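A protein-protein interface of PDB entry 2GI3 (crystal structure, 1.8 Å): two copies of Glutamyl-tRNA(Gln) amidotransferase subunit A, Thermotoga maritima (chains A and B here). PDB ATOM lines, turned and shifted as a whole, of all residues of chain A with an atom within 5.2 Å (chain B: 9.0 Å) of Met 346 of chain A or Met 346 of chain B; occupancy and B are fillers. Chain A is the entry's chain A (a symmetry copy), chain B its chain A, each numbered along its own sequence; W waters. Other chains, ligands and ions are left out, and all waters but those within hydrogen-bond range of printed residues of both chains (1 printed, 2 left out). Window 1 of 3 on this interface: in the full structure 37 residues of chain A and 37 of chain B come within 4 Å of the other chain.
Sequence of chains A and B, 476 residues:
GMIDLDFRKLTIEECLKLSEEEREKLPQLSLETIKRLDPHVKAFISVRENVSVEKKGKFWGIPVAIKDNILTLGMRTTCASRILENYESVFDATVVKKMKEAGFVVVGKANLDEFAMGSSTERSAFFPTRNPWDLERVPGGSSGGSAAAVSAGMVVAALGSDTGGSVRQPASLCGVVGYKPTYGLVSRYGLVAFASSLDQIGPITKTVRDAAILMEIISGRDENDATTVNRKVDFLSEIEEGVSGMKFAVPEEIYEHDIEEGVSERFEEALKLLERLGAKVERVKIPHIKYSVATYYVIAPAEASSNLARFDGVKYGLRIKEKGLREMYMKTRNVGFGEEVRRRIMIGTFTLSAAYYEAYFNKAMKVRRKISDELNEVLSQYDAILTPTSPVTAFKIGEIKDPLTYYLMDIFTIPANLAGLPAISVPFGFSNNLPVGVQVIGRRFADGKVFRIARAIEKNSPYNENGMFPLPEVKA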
ATOM      1  N   VAL A 341     -19.716 -27.544  19.964  1.00  0.00           N
ATOM      2  CA  VAL A 341     -20.345 -27.045  18.757  1.00  0.00           C
ATOM      3  C   VAL A 341     -20.738 -25.586  18.977  1.00  0.00           C
ATOM      4  O   VAL A 341     -20.524 -24.761  18.102  1.00  0.00           O
ATOM      5  CB  VAL A 341     -21.579 -27.870  18.361  1.00  0.00           C
ATOM      6  CG1 VAL A 341     -22.287 -27.200  17.193  1.00  0.00           C
ATOM      7  CG2 VAL A 341     -21.181 -29.309  18.008  1.00  0.00           C
ATOM      8  N   ARG A 342     -21.301 -25.274  20.145  1.00  0.00           N
ATOM      9  CA  ARG A 342     -21.669 -23.894  20.470  1.00  0.00           C
ATOM     10  C   ARG A 342     -20.426 -22.992  20.510  1.00  0.00           C
ATOM     11  O   ARG A 342     -20.434 -21.890  19.962  1.00  0.00           O
ATOM     12  CB  ARG A 342     -22.434 -23.827  21.797  1.00  0.00           C
ATOM     13  CG  ARG A 342     -23.034 -22.444  22.095  1.00  0.00           C
ATOM     14  CD  ARG A 342     -24.133 -22.484  23.160  1.00  0.00           C
ATOM     15  NE  ARG A 342     -25.316 -23.254  22.734  1.00  0.00           N
ATOM     16  CZ  ARG A 342     -25.601 -24.515  23.088  1.00  0.00           C
ATOM     17  NH1 ARG A 342     -24.800 -25.218  23.892  1.00  0.00           N
ATOM     18  NH2 ARG A 342     -26.708 -25.089  22.624  1.00  0.00           N
ATOM     19  N   ARG A 343     -19.361 -23.475  21.146  1.00  0.00           N
ATOM     20  CA  ARG A 343     -18.080 -22.773  21.176  1.00  0.00           C
ATOM     21  C   ARG A 343     -17.578 -22.456  19.785  1.00  0.00           C
ATOM     22  O   ARG A 343     -17.208 -21.320  19.503  1.00  0.00           O
ATOM     23  CB  ARG A 343     -17.006 -23.625  21.862  1.00  0.00           C
ATOM     24  CG  ARG A 343     -17.013 -23.566  23.371  1.00  0.00           C
ATOM     25  CD  ARG A 343     -15.810 -24.346  23.948  1.00  0.00           C
ATOM     26  NE  ARG A 343     -16.137 -24.912  25.256  1.00  0.00           N
ATOM     27  CZ  ARG A 343     -16.168 -24.224  26.398  1.00  0.00           C
ATOM     28  NH1 ARG A 343     -15.889 -22.920  26.421  1.00  0.00           N
ATOM     29  NH2 ARG A 343     -16.490 -24.842  27.530  1.00  0.00           N
ATOM     30  N   ARG A 344     -17.532 -23.468  18.927  1.00  0.00           N
ATOM     31  CA  ARG A 344     -17.005 -23.278  17.584  1.00  0.00           C
ATOM     32  C   ARG A 344     -17.847 -22.251  16.836  1.00  0.00           C
ATOM     33  O   ARG A 344     -17.313 -21.363  16.169  1.00  0.00           O
ATOM     34  CB  ARG A 344     -16.907 -24.597  16.793  1.00  0.00           C
ATOM     35  CG  ARG A 344     -15.614 -25.396  17.028  1.00  0.00           C
ATOM     36  CD  ARG A 344     -14.314 -24.642  16.604  1.00  0.00           C
ATOM     37  NE  ARG A 344     -14.294 -24.166  15.202  1.00  0.00           N
ATOM     38  CZ  ARG A 344     -14.464 -22.899  14.792  1.00  0.00           C
ATOM     39  NH1 ARG A 344     -14.674 -21.911  15.655  1.00  0.00           N
ATOM     40  NH2 ARG A 344     -14.425 -22.598  13.498  1.00  0.00           N
ATOM     41  N   ILE A 345     -19.161 -22.364  16.976  1.00  0.00           N
ATOM     42  CA  ILE A 345     -20.072 -21.450  16.294  1.00  0.00           C
ATOM     43  C   ILE A 345     -19.885 -20.027  16.830  1.00  0.00           C
ATOM     44  O   ILE A 345     -19.878 -19.057  16.062  1.00  0.00           O
ATOM     45  CB  ILE A 345     -21.530 -21.889  16.444  1.00  0.00           C
ATOM     46  CG1 ILE A 345     -21.767 -23.216  15.699  1.00  0.00           C
ATOM     47  CG2 ILE A 345     -22.462 -20.770  15.954  1.00  0.00           C
ATOM     48  CD1 ILE A 345     -22.144 -23.079  14.224  1.00  0.00           C
ATOM     49  N   MET A 346     -19.707 -19.908  18.140  1.00  0.00           N
ATOM     50  CA  MET A 346     -19.531 -18.610  18.743  1.00  0.00           C
ATOM     51  C   MET A 346     -18.221 -17.955  18.323  1.00  0.00           C
ATOM     52  O   MET A 346     -18.188 -16.767  18.007  1.00  0.00           O
ATOM     53  CB  MET A 346     -19.583 -18.717  20.252  1.00  0.00           C
ATOM     54  CG  MET A 346     -19.768 -17.361  20.898  1.00  0.00           C
ATOM     55  SD  MET A 346     -20.483 -17.504  22.680  1.00  0.00           S
ATOM     56  CE  MET A 346     -21.753 -18.948  22.385  1.00  0.00           C
ATOM     57  N   ILE A 347     -17.142 -18.725  18.305  1.00  0.00           N
ATOM     58  CA  ILE A 347     -15.858 -18.200  17.864  1.00  0.00           C
ATOM     59  C   ILE A 347     -15.931 -17.851  16.376  1.00  0.00           C
ATOM     60  O   ILE A 347     -15.376 -16.840  15.930  1.00  0.00           O
ATOM     61  CB  ILE A 347     -14.701 -19.214  18.078  1.00  0.00           C
ATOM     62  CG1 ILE A 347     -14.498 -19.521  19.564  1.00  0.00           C
ATOM     63  CG2 ILE A 347     -13.408 -18.660  17.520  1.00  0.00           C
ATOM     64  CD1 ILE A 347     -13.644 -20.775  19.792  1.00  0.00           C
ATOM     65  N   GLY A 348     -16.613 -18.709  15.614  1.00  0.00           N
ATOM     66  CA  GLY A 348     -16.827 -18.493  14.185  1.00  0.00           C
ATOM     67  C   GLY A 348     -17.582 -17.208  13.898  1.00  0.00           C
ATOM     68  O   GLY A 348     -17.168 -16.415  13.044  1.00  0.00           O
ATOM     69  N   THR A 349     -18.686 -17.013  14.613  1.00  0.00           N
ATOM     70  CA  THR A 349     -19.479 -15.786  14.501  1.00  0.00           C
ATOM     71  C   THR A 349     -18.667 -14.538  14.837  1.00  0.00           C
ATOM     72  O   THR A 349     -18.820 -13.477  14.208  1.00  0.00           O
ATOM     73  CB  THR A 349     -20.711 -15.859  15.400  1.00  0.00           C
ATOM     74  OG1 THR A 349     -21.419 -17.051  15.066  1.00  0.00           O
ATOM     75  CG2 THR A 349     -21.633 -14.664  15.170  1.00  0.00           C
ATOM     76  N   PHE A 350     -17.785 -14.671  15.813  1.00  0.00           N
ATOM     77  CA  PHE A 350     -16.985 -13.553  16.203  1.00  0.00           C
ATOM     78  C   PHE A 350     -16.036 -13.122  15.087  1.00  0.00           C
ATOM     79  O   PHE A 350     -15.881 -11.934  14.819  1.00  0.00           O
ATOM     80  CB  PHE A 350     -16.204 -13.862  17.465  1.00  0.00           C
ATOM     81  CG  PHE A 350     -15.472 -12.672  17.985  1.00  0.00           C
ATOM     82  CD1 PHE A 350     -16.191 -11.597  18.521  1.00  0.00           C
ATOM     83  CD2 PHE A 350     -14.090 -12.577  17.869  1.00  0.00           C
ATOM     84  CE1 PHE A 350     -15.543 -10.462  18.974  1.00  0.00           C
ATOM     85  CE2 PHE A 350     -13.419 -11.441  18.327  1.00  0.00           C
ATOM     86  CZ  PHE A 350     -14.150 -10.380  18.885  1.00  0.00           C
ATOM     87  N   MET B 117     -15.815 -25.871   8.967  1.00  0.00           N
ATOM     88  CA  MET B 117     -15.964 -24.433   9.039  1.00  0.00           C
ATOM     89  C   MET B 117     -14.629 -23.779   8.743  1.00  0.00           C
ATOM     90  O   MET B 117     -13.948 -23.329   9.650  1.00  0.00           O
ATOM     91  CB  MET B 117     -16.497 -24.020  10.413  1.00  0.00           C
ATOM     92  CG  MET B 117     -17.896 -24.517  10.699  1.00  0.00           C
ATOM     93  SD  MET B 117     -18.414 -24.357  12.593  1.00  0.00           S
ATOM     94  CE  MET B 117     -20.248 -25.031  12.373  1.00  0.00           C
ATOM     95  N   ALA B 304     -26.401 -22.672  10.176  1.00  0.00           N
ATOM     96  CA  ALA B 304     -25.542 -23.354  11.171  1.00  0.00           C
ATOM     97  C   ALA B 304     -26.056 -23.221  12.617  1.00  0.00           C
ATOM     98  O   ALA B 304     -26.155 -24.213  13.350  1.00  0.00           O
ATOM     99  CB  ALA B 304     -24.160 -22.825  11.072  1.00  0.00           C
ATOM    100  N   SER B 305     -26.389 -21.980  12.988  1.00  0.00           N
ATOM    101  CA  SER B 305     -26.948 -21.636  14.305  1.00  0.00           C
ATOM    102  C   SER B 305     -28.344 -22.230  14.494  1.00  0.00           C
ATOM    103  O   SER B 305     -28.751 -22.509  15.614  1.00  0.00           O
ATOM    104  CB  SER B 305     -26.976 -20.109  14.501  1.00  0.00           C
ATOM    105  OG  SER B 305     -25.687 -19.530  14.258  1.00  0.00           O
ATOM    106  N   GLY B 338      -8.812  -8.983  30.766  1.00  0.00           N
ATOM    107  CA  GLY B 338      -8.860  -9.188  29.323  1.00  0.00           C
ATOM    108  C   GLY B 338      -9.796 -10.309  28.907  1.00  0.00           C
ATOM    109  O   GLY B 338     -10.622 -10.124  28.012  1.00  0.00           O
ATOM    110  N   GLU B 339      -9.675 -11.466  29.560  1.00  0.00           N
ATOM    111  CA  GLU B 339     -10.499 -12.640  29.212  1.00  0.00           C
ATOM    112  C   GLU B 339     -11.988 -12.386  29.403  1.00  0.00           C
ATOM    113  O   GLU B 339     -12.792 -12.809  28.572  1.00  0.00           O
ATOM    114  CB  GLU B 339     -10.098 -13.877  30.019  1.00  0.00           C
ATOM    115  N   GLU B 340     -12.350 -11.706  30.490  1.00  0.00           N
ATOM    116  CA  GLU B 340     -13.755 -11.422  30.786  1.00  0.00           C
ATOM    117  C   GLU B 340     -14.342 -10.445  29.765  1.00  0.00           C
ATOM    118  O   GLU B 340     -15.507 -10.585  29.345  1.00  0.00           O
ATOM    119  CB  GLU B 340     -13.923 -10.846  32.216  1.00  0.00           C
ATOM    120  CG  GLU B 340     -15.349 -10.328  32.566  1.00  0.00           C
ATOM    121  CD  GLU B 340     -16.457 -11.390  32.384  1.00  0.00           C
ATOM    122  OE1 GLU B 340     -16.137 -12.592  32.299  1.00  0.00           O
ATOM    123  OE2 GLU B 340     -17.657 -11.022  32.321  1.00  0.00           O
ATOM    124  N   VAL B 341     -13.546  -9.442  29.396  1.00  0.00           N
ATOM    125  CA  VAL B 341     -13.994  -8.447  28.442  1.00  0.00           C
ATOM    126  C   VAL B 341     -14.170  -9.118  27.082  1.00  0.00           C
ATOM    127  O   VAL B 341     -15.157  -8.872  26.407  1.00  0.00           O
ATOM    128  CB  VAL B 341     -13.015  -7.269  28.326  1.00  0.00           C
ATOM    129  CG1 VAL B 341     -13.454  -6.350  27.196  1.00  0.00           C
ATOM    130  CG2 VAL B 341     -12.928  -6.502  29.653  1.00  0.00           C
ATOM    131  N   ARG B 342     -13.219  -9.967  26.692  1.00  0.00           N
ATOM    132  CA  ARG B 342     -13.321 -10.698  25.426  1.00  0.00           C
ATOM    133  C   ARG B 342     -14.542 -11.629  25.428  1.00  0.00           C
ATOM    134  O   ARG B 342     -15.293 -11.679  24.454  1.00  0.00           O
ATOM    135  CB  ARG B 342     -12.036 -11.484  25.140  1.00  0.00           C
ATOM    136  CG  ARG B 342     -11.988 -12.101  23.734  1.00  0.00           C
ATOM    137  CD  ARG B 342     -10.575 -12.496  23.299  1.00  0.00           C
ATOM    138  NE  ARG B 342      -9.672 -11.339  23.165  1.00  0.00           N
ATOM    139  CZ  ARG B 342      -8.761 -10.945  24.065  1.00  0.00           C
ATOM    140  NH1 ARG B 342      -8.586 -11.595  25.219  1.00  0.00           N
ATOM    141  NH2 ARG B 342      -8.012  -9.876  23.812  1.00  0.00           N
ATOM    142  N   ARG B 343     -14.740 -12.347  26.531  1.00  0.00           N
ATOM    143  CA  ARG B 343     -15.915 -13.196  26.714  1.00  0.00           C
ATOM    144  C   ARG B 343     -17.202 -12.425  26.530  1.00  0.00           C
ATOM    145  O   ARG B 343     -18.082 -12.855  25.790  1.00  0.00           O
ATOM    146  CB  ARG B 343     -15.943 -13.794  28.126  1.00  0.00           C
ATOM    147  CG  ARG B 343     -15.089 -15.026  28.313  1.00  0.00           C
ATOM    148  CD  ARG B 343     -15.300 -15.619  29.725  1.00  0.00           C
ATOM    149  NE  ARG B 343     -14.085 -16.284  30.196  1.00  0.00           N
ATOM    150  CZ  ARG B 343     -13.679 -17.492  29.808  1.00  0.00           C
ATOM    151  NH1 ARG B 343     -14.384 -18.205  28.929  1.00  0.00           N
ATOM    152  NH2 ARG B 343     -12.548 -17.994  30.297  1.00  0.00           N
ATOM    153  N   ARG B 344     -17.326 -11.304  27.231  1.00  0.00           N
ATOM    154  CA  ARG B 344     -18.553 -10.525  27.170  1.00  0.00           C
ATOM    155  C   ARG B 344     -18.796 -10.048  25.743  1.00  0.00           C
ATOM    156  O   ARG B 344     -19.916 -10.124  25.235  1.00  0.00           O
ATOM    157  CB  ARG B 344     -18.553  -9.341  28.158  1.00  0.00           C
ATOM    158  CG  ARG B 344     -19.019  -9.688  29.582  1.00  0.00           C
ATOM    159  CD  ARG B 344     -20.491 -10.205  29.662  1.00  0.00           C
ATOM    160  NE  ARG B 344     -21.505  -9.303  29.070  1.00  0.00           N
ATOM    161  CZ  ARG B 344     -22.127  -9.473  27.892  1.00  0.00           C
ATOM    162  NH1 ARG B 344     -21.873 -10.521  27.118  1.00  0.00           N
ATOM    163  NH2 ARG B 344     -23.022  -8.587  27.469  1.00  0.00           N
ATOM    164  N   ILE B 345     -17.735  -9.585  25.096  1.00  0.00           N
ATOM    165  CA  ILE B 345     -17.846  -9.084  23.730  1.00  0.00           C
ATOM    166  C   ILE B 345     -18.238 -10.223  22.784  1.00  0.00           C
ATOM    167  O   ILE B 345     -19.074 -10.045  21.889  1.00  0.00           O
ATOM    168  CB  ILE B 345     -16.546  -8.425  23.263  1.00  0.00           C
ATOM    169  CG1 ILE B 345     -16.278  -7.141  24.070  1.00  0.00           C
ATOM    170  CG2 ILE B 345     -16.612  -8.160  21.751  1.00  0.00           C
ATOM    171  CD1 ILE B 345     -16.917  -5.871  23.509  1.00  0.00           C
ATOM    172  N   MET B 346     -17.655 -11.396  22.999  1.00  0.00           N
ATOM    173  CA  MET B 346     -17.950 -12.529  22.157  1.00  0.00           C
ATOM    174  C   MET B 346     -19.386 -13.008  22.323  1.00  0.00           C
ATOM    175  O   MET B 346     -20.068 -13.299  21.341  1.00  0.00           O
ATOM    176  CB  MET B 346     -16.998 -13.668  22.452  1.00  0.00           C
ATOM    177  CG  MET B 346     -17.035 -14.717  21.362  1.00  0.00           C
ATOM    178  SD  MET B 346     -15.439 -15.795  21.345  1.00  0.00           S
ATOM    179  CE  MET B 346     -14.129 -14.407  21.720  1.00  0.00           C
ATOM    180  N   ILE B 347     -19.858 -13.081  23.560  1.00  0.00           N
ATOM    181  CA  ILE B 347     -21.236 -13.475  23.812  1.00  0.00           C
ATOM    182  C   ILE B 347     -22.183 -12.410  23.255  1.00  0.00           C
ATOM    183  O   ILE B 347     -23.240 -12.727  22.696  1.00  0.00           O
ATOM    184  CB  ILE B 347     -21.531 -13.656  25.326  1.00  0.00           C
ATOM    185  CG1 ILE B 347     -20.694 -14.789  25.925  1.00  0.00           C
ATOM    186  CG2 ILE B 347     -22.995 -13.972  25.542  1.00  0.00           C
ATOM    187  CD1 ILE B 347     -20.670 -14.752  27.459  1.00  0.00           C
ATOM    188  N   GLY B 348     -21.795 -11.145  23.426  1.00  0.00           N
ATOM    189  CA  GLY B 348     -22.555 -10.012  22.904  1.00  0.00           C
ATOM    190  C   GLY B 348     -22.697 -10.055  21.393  1.00  0.00           C
ATOM    191  O   GLY B 348     -23.802  -9.890  20.862  1.00  0.00           O
ATOM    192  N   THR B 349     -21.575 -10.273  20.713  1.00  0.00           N
ATOM    193  CA  THR B 349     -21.566 -10.415  19.254  1.00  0.00           C
ATOM    194  C   THR B 349     -22.448 -11.566  18.778  1.00  0.00           C
ATOM    195  O   THR B 349     -23.127 -11.475  17.740  1.00  0.00           O
ATOM    196  CB  THR B 349     -20.141 -10.611  18.743  1.00  0.00           C
ATOM    197  OG1 THR B 349     -19.353  -9.528  19.235  1.00  0.00           O
ATOM    198  CG2 THR B 349     -20.095 -10.592  17.217  1.00  0.00           C
ATOM    199  N   PHE B 350     -22.459 -12.640  19.548  1.00  0.00           N
ATOM    200  CA  PHE B 350     -23.250 -13.771  19.177  1.00  0.00           C
ATOM    201  C   PHE B 350     -24.741 -13.449  19.204  1.00  0.00           C
ATOM    202  O   PHE B 350     -25.482 -13.827  18.299  1.00  0.00           O
ATOM    203  CB  PHE B 350     -22.953 -14.955  20.076  1.00  0.00           C
ATOM    204  CG  PHE B 350     -23.649 -16.196  19.629  1.00  0.00           C
ATOM    205  CD1 PHE B 350     -23.257 -16.818  18.437  1.00  0.00           C
ATOM    206  CD2 PHE B 350     -24.737 -16.697  20.333  1.00  0.00           C
ATOM    207  CE1 PHE B 350     -23.909 -17.946  17.975  1.00  0.00           C
ATOM    208  CE2 PHE B 350     -25.404 -17.840  19.883  1.00  0.00           C
ATOM    209  CZ  PHE B 350     -24.984 -18.467  18.700  1.00  0.00           C
ATOM    210  N   THR B 351     -25.181 -12.763  20.252  1.00  0.00           N
ATOM    211  CA  THR B 351     -26.592 -12.400  20.395  1.00  0.00           C
ATOM    212  C   THR B 351     -26.980 -11.363  19.342  1.00  0.00           C
ATOM    213  O   THR B 351     -28.059 -11.400  18.770  1.00  0.00           O
ATOM    214  CB  THR B 351     -26.856 -11.836  21.829  1.00  0.00           C
ATOM    215  OG1 THR B 351     -26.401 -12.802  22.791  1.00  0.00           O
ATOM    216  CG2 THR B 351     -28.309 -11.552  22.060  1.00  0.00           C
ATOM    217  N   LEU B 352     -26.073 -10.445  19.076  1.00  0.00           N
ATOM    218  CA  LEU B 352     -26.347  -9.445  18.051  1.00  0.00           C
ATOM    219  C   LEU B 352     -26.463 -10.095  16.653  1.00  0.00           C
ATOM    220  O   LEU B 352     -27.295  -9.675  15.843  1.00  0.00           O
ATOM    221  CB  LEU B 352     -25.257  -8.401  18.047  1.00  0.00           C
ATOM    222  CG  LEU B 352     -25.510  -7.047  17.399  1.00  0.00           C
ATOM    223  CD1 LEU B 352     -26.912  -6.563  17.692  1.00  0.00           C
ATOM    224  CD2 LEU B 352     -24.436  -6.076  17.928  1.00  0.00           C
ATOM    225  N   SER B 353     -25.628 -11.099  16.381  1.00  0.00           N
ATOM    226  CA  SER B 353     -25.663 -11.797  15.086  1.00  0.00           C
ATOM    227  C   SER B 353     -26.987 -12.501  14.950  1.00  0.00           C
ATOM    228  O   SER B 353     -27.558 -12.516  13.869  1.00  0.00           O
ATOM    229  CB  SER B 353     -24.528 -12.816  14.957  1.00  0.00           C
ATOM    230  OG  SER B 353     -23.281 -12.152  15.082  1.00  0.00           O
ATOM    231  N   TYR B 357     -29.649 -12.109  11.886  1.00  0.00           N
ATOM    232  CA  TYR B 357     -30.263 -13.207  11.113  1.00  0.00           C
ATOM    233  C   TYR B 357     -31.767 -13.071  11.142  1.00  0.00           C
ATOM    234  O   TYR B 357     -32.431 -13.185  10.113  1.00  0.00           O
ATOM    235  CB  TYR B 357     -29.861 -14.600  11.609  1.00  0.00           C
ATOM    236  CG  TYR B 357     -28.365 -14.865  11.676  1.00  0.00           C
ATOM    237  CD1 TYR B 357     -27.478 -14.257  10.795  1.00  0.00           C
ATOM    238  CD2 TYR B 357     -27.834 -15.746  12.636  1.00  0.00           C
ATOM    239  CE1 TYR B 357     -26.102 -14.501  10.864  1.00  0.00           C
ATOM    240  CE2 TYR B 357     -26.464 -15.992  12.720  1.00  0.00           C
ATOM    241  CZ  TYR B 357     -25.601 -15.364  11.824  1.00  0.00           C
ATOM    242  OH  TYR B 357     -24.235 -15.579  11.868  1.00  0.00           O
ATOM    243  N   TYR B 407     -12.341 -14.682   4.476  1.00  0.00           N
ATOM    244  CA  TYR B 407     -13.706 -14.957   4.053  1.00  0.00           C
ATOM    245  C   TYR B 407     -14.000 -14.589   2.608  1.00  0.00           C
ATOM    246  O   TYR B 407     -15.036 -14.967   2.072  1.00  0.00           O
ATOM    247  CB  TYR B 407     -14.682 -14.309   5.017  1.00  0.00           C
ATOM    248  CG  TYR B 407     -14.709 -15.013   6.342  1.00  0.00           C
ATOM    249  CD1 TYR B 407     -15.136 -16.332   6.423  1.00  0.00           C
ATOM    250  CD2 TYR B 407     -14.320 -14.374   7.514  1.00  0.00           C
ATOM    251  CE1 TYR B 407     -15.195 -17.004   7.647  1.00  0.00           C
ATOM    252  CE2 TYR B 407     -14.356 -15.042   8.747  1.00  0.00           C
ATOM    253  CZ  TYR B 407     -14.795 -16.361   8.800  1.00  0.00           C
ATOM    254  OH  TYR B 407     -14.839 -17.060   9.993  1.00  0.00           O
HETATM  255  O   HOH W   1     -13.512 -24.917  11.712  1.00  0.00           O
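O of Ile 345 of chain B is in hydrogen-bond range of OG1 of Thr 349 of chain B (2.7 Å). The backbone carbonyl oxygen of Thr 349 of chain B sits at hydrogen-bond distance from the side-chain hydroxyl of Ser 353 of chain B, 2.7 Å away. The backbone carbonyl oxygen (O) of Ile 345 of chain A lies within hydrogen-bond range of the side-chain hydroxyl (OG1) of Thr 349 of chain A (2.7 Å).
Of chain B, only Met 346 (3.8 Å) comes within 4 Å of Met 346 of chain A. Of chain A, only Met 346 comes within 4 Å of Met 346 of chain B. Of the printed residues of chain A, Ala 304 of chain B touches Ile 345 (3.8 Å). Of the printed residues of chain B, Arg 344 of chain A touches Met 117 (3.9 Å). Printed residues of chain B within 4 Å of Thr 349 of chain A: Phe 350 (3.8 Å) and Ser 353 (3.0 Å). Printed residues of chain A within 4 Å of Ser 353 of chain B: Thr 349. Of the printed residues of chain B, Ile 345 of chain A touches Met 117 (3.3 Å), Ala 304 (3.8 Å), Ser 305 (3.8 Å) and Phe 350 (3.8 Å). Arg 343 of chain B touches none of the printed residues of chain A. Gly 338 of chain B touches none of the printed residues of chain A. The nearest residue of chain B that does not touch Met 346 of chain A is Phe 350 of chain B (4.1 Å). The nearest residue of chain A that does not touch Met 346 of chain B is Phe 350 of chain A (4.1 Å).
Printed residues of chain B that touch a printed residue of chain A: Met 117, Ala 304, Ser 305, Ile 345, Met 346, Thr 349, Phe 350, Ser 353 and Tyr 407. Hydrophobic or aromatic side chains of chain A within 4 Å of the printed part of chain B: Ile 345, Met 346 and Phe 350. Among the printed residues, 11 pairs touch across the chains.
Water W1 bridges the backbone carbonyl oxygen of Met 117 of chain B (2.6 Å) and the guanidinium group of Arg 344 of chain A (3.1 Å).
Ile 345 of chain A touches Met 117 of chain B. CD1 of Ile 345 of chain A touches CB of Ala 304 of chain B, 3.8 Å away. Ile 345 of chain A touches Ser 305 of chain B. Phe 350 of chain B touches Ile 345 of chain A (CE1 to CG2, 3.8 Å). Met 346 of chain A touches Met 346 of chain B (CG to CG, 3.8 Å). O of Gly 348 of chain A touches OH of Tyr 407 of chain B, at 3.9 Å. OG1 of Thr 349 of chain A touches CD1 of Phe 350 of chain B, 3.8 Å away. CG2 of Thr 349 of chain A touches OG of Ser 353 of chain B (3.0 Å). CE1 of Phe 350 of chain A touches CG2 of Ile 345 of chain B, 3.8 Å away. Phe 350 of chain A touches Thr 349 of chain B.
Ile 345 of chain A touches Phe 350 of chain B, and with the chains exchanged Phe 350 of chain A touches Ile 345 of chain B. Met 346 of chain B touches its own counterpart, Met 346 of chain A. Thr 349 of chain A touches Phe 350 of chain B, and with the chains exchanged Phe 350 of chain A touches Thr 349 of chain B. Positions printed for both chains: 341, 342, 343, 344, 345, 346, 347, 348, 349 and 350. Of the 11 pairs that touch across the chains among the printed residues, 5 have their exchanged pair printed and touching as well.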
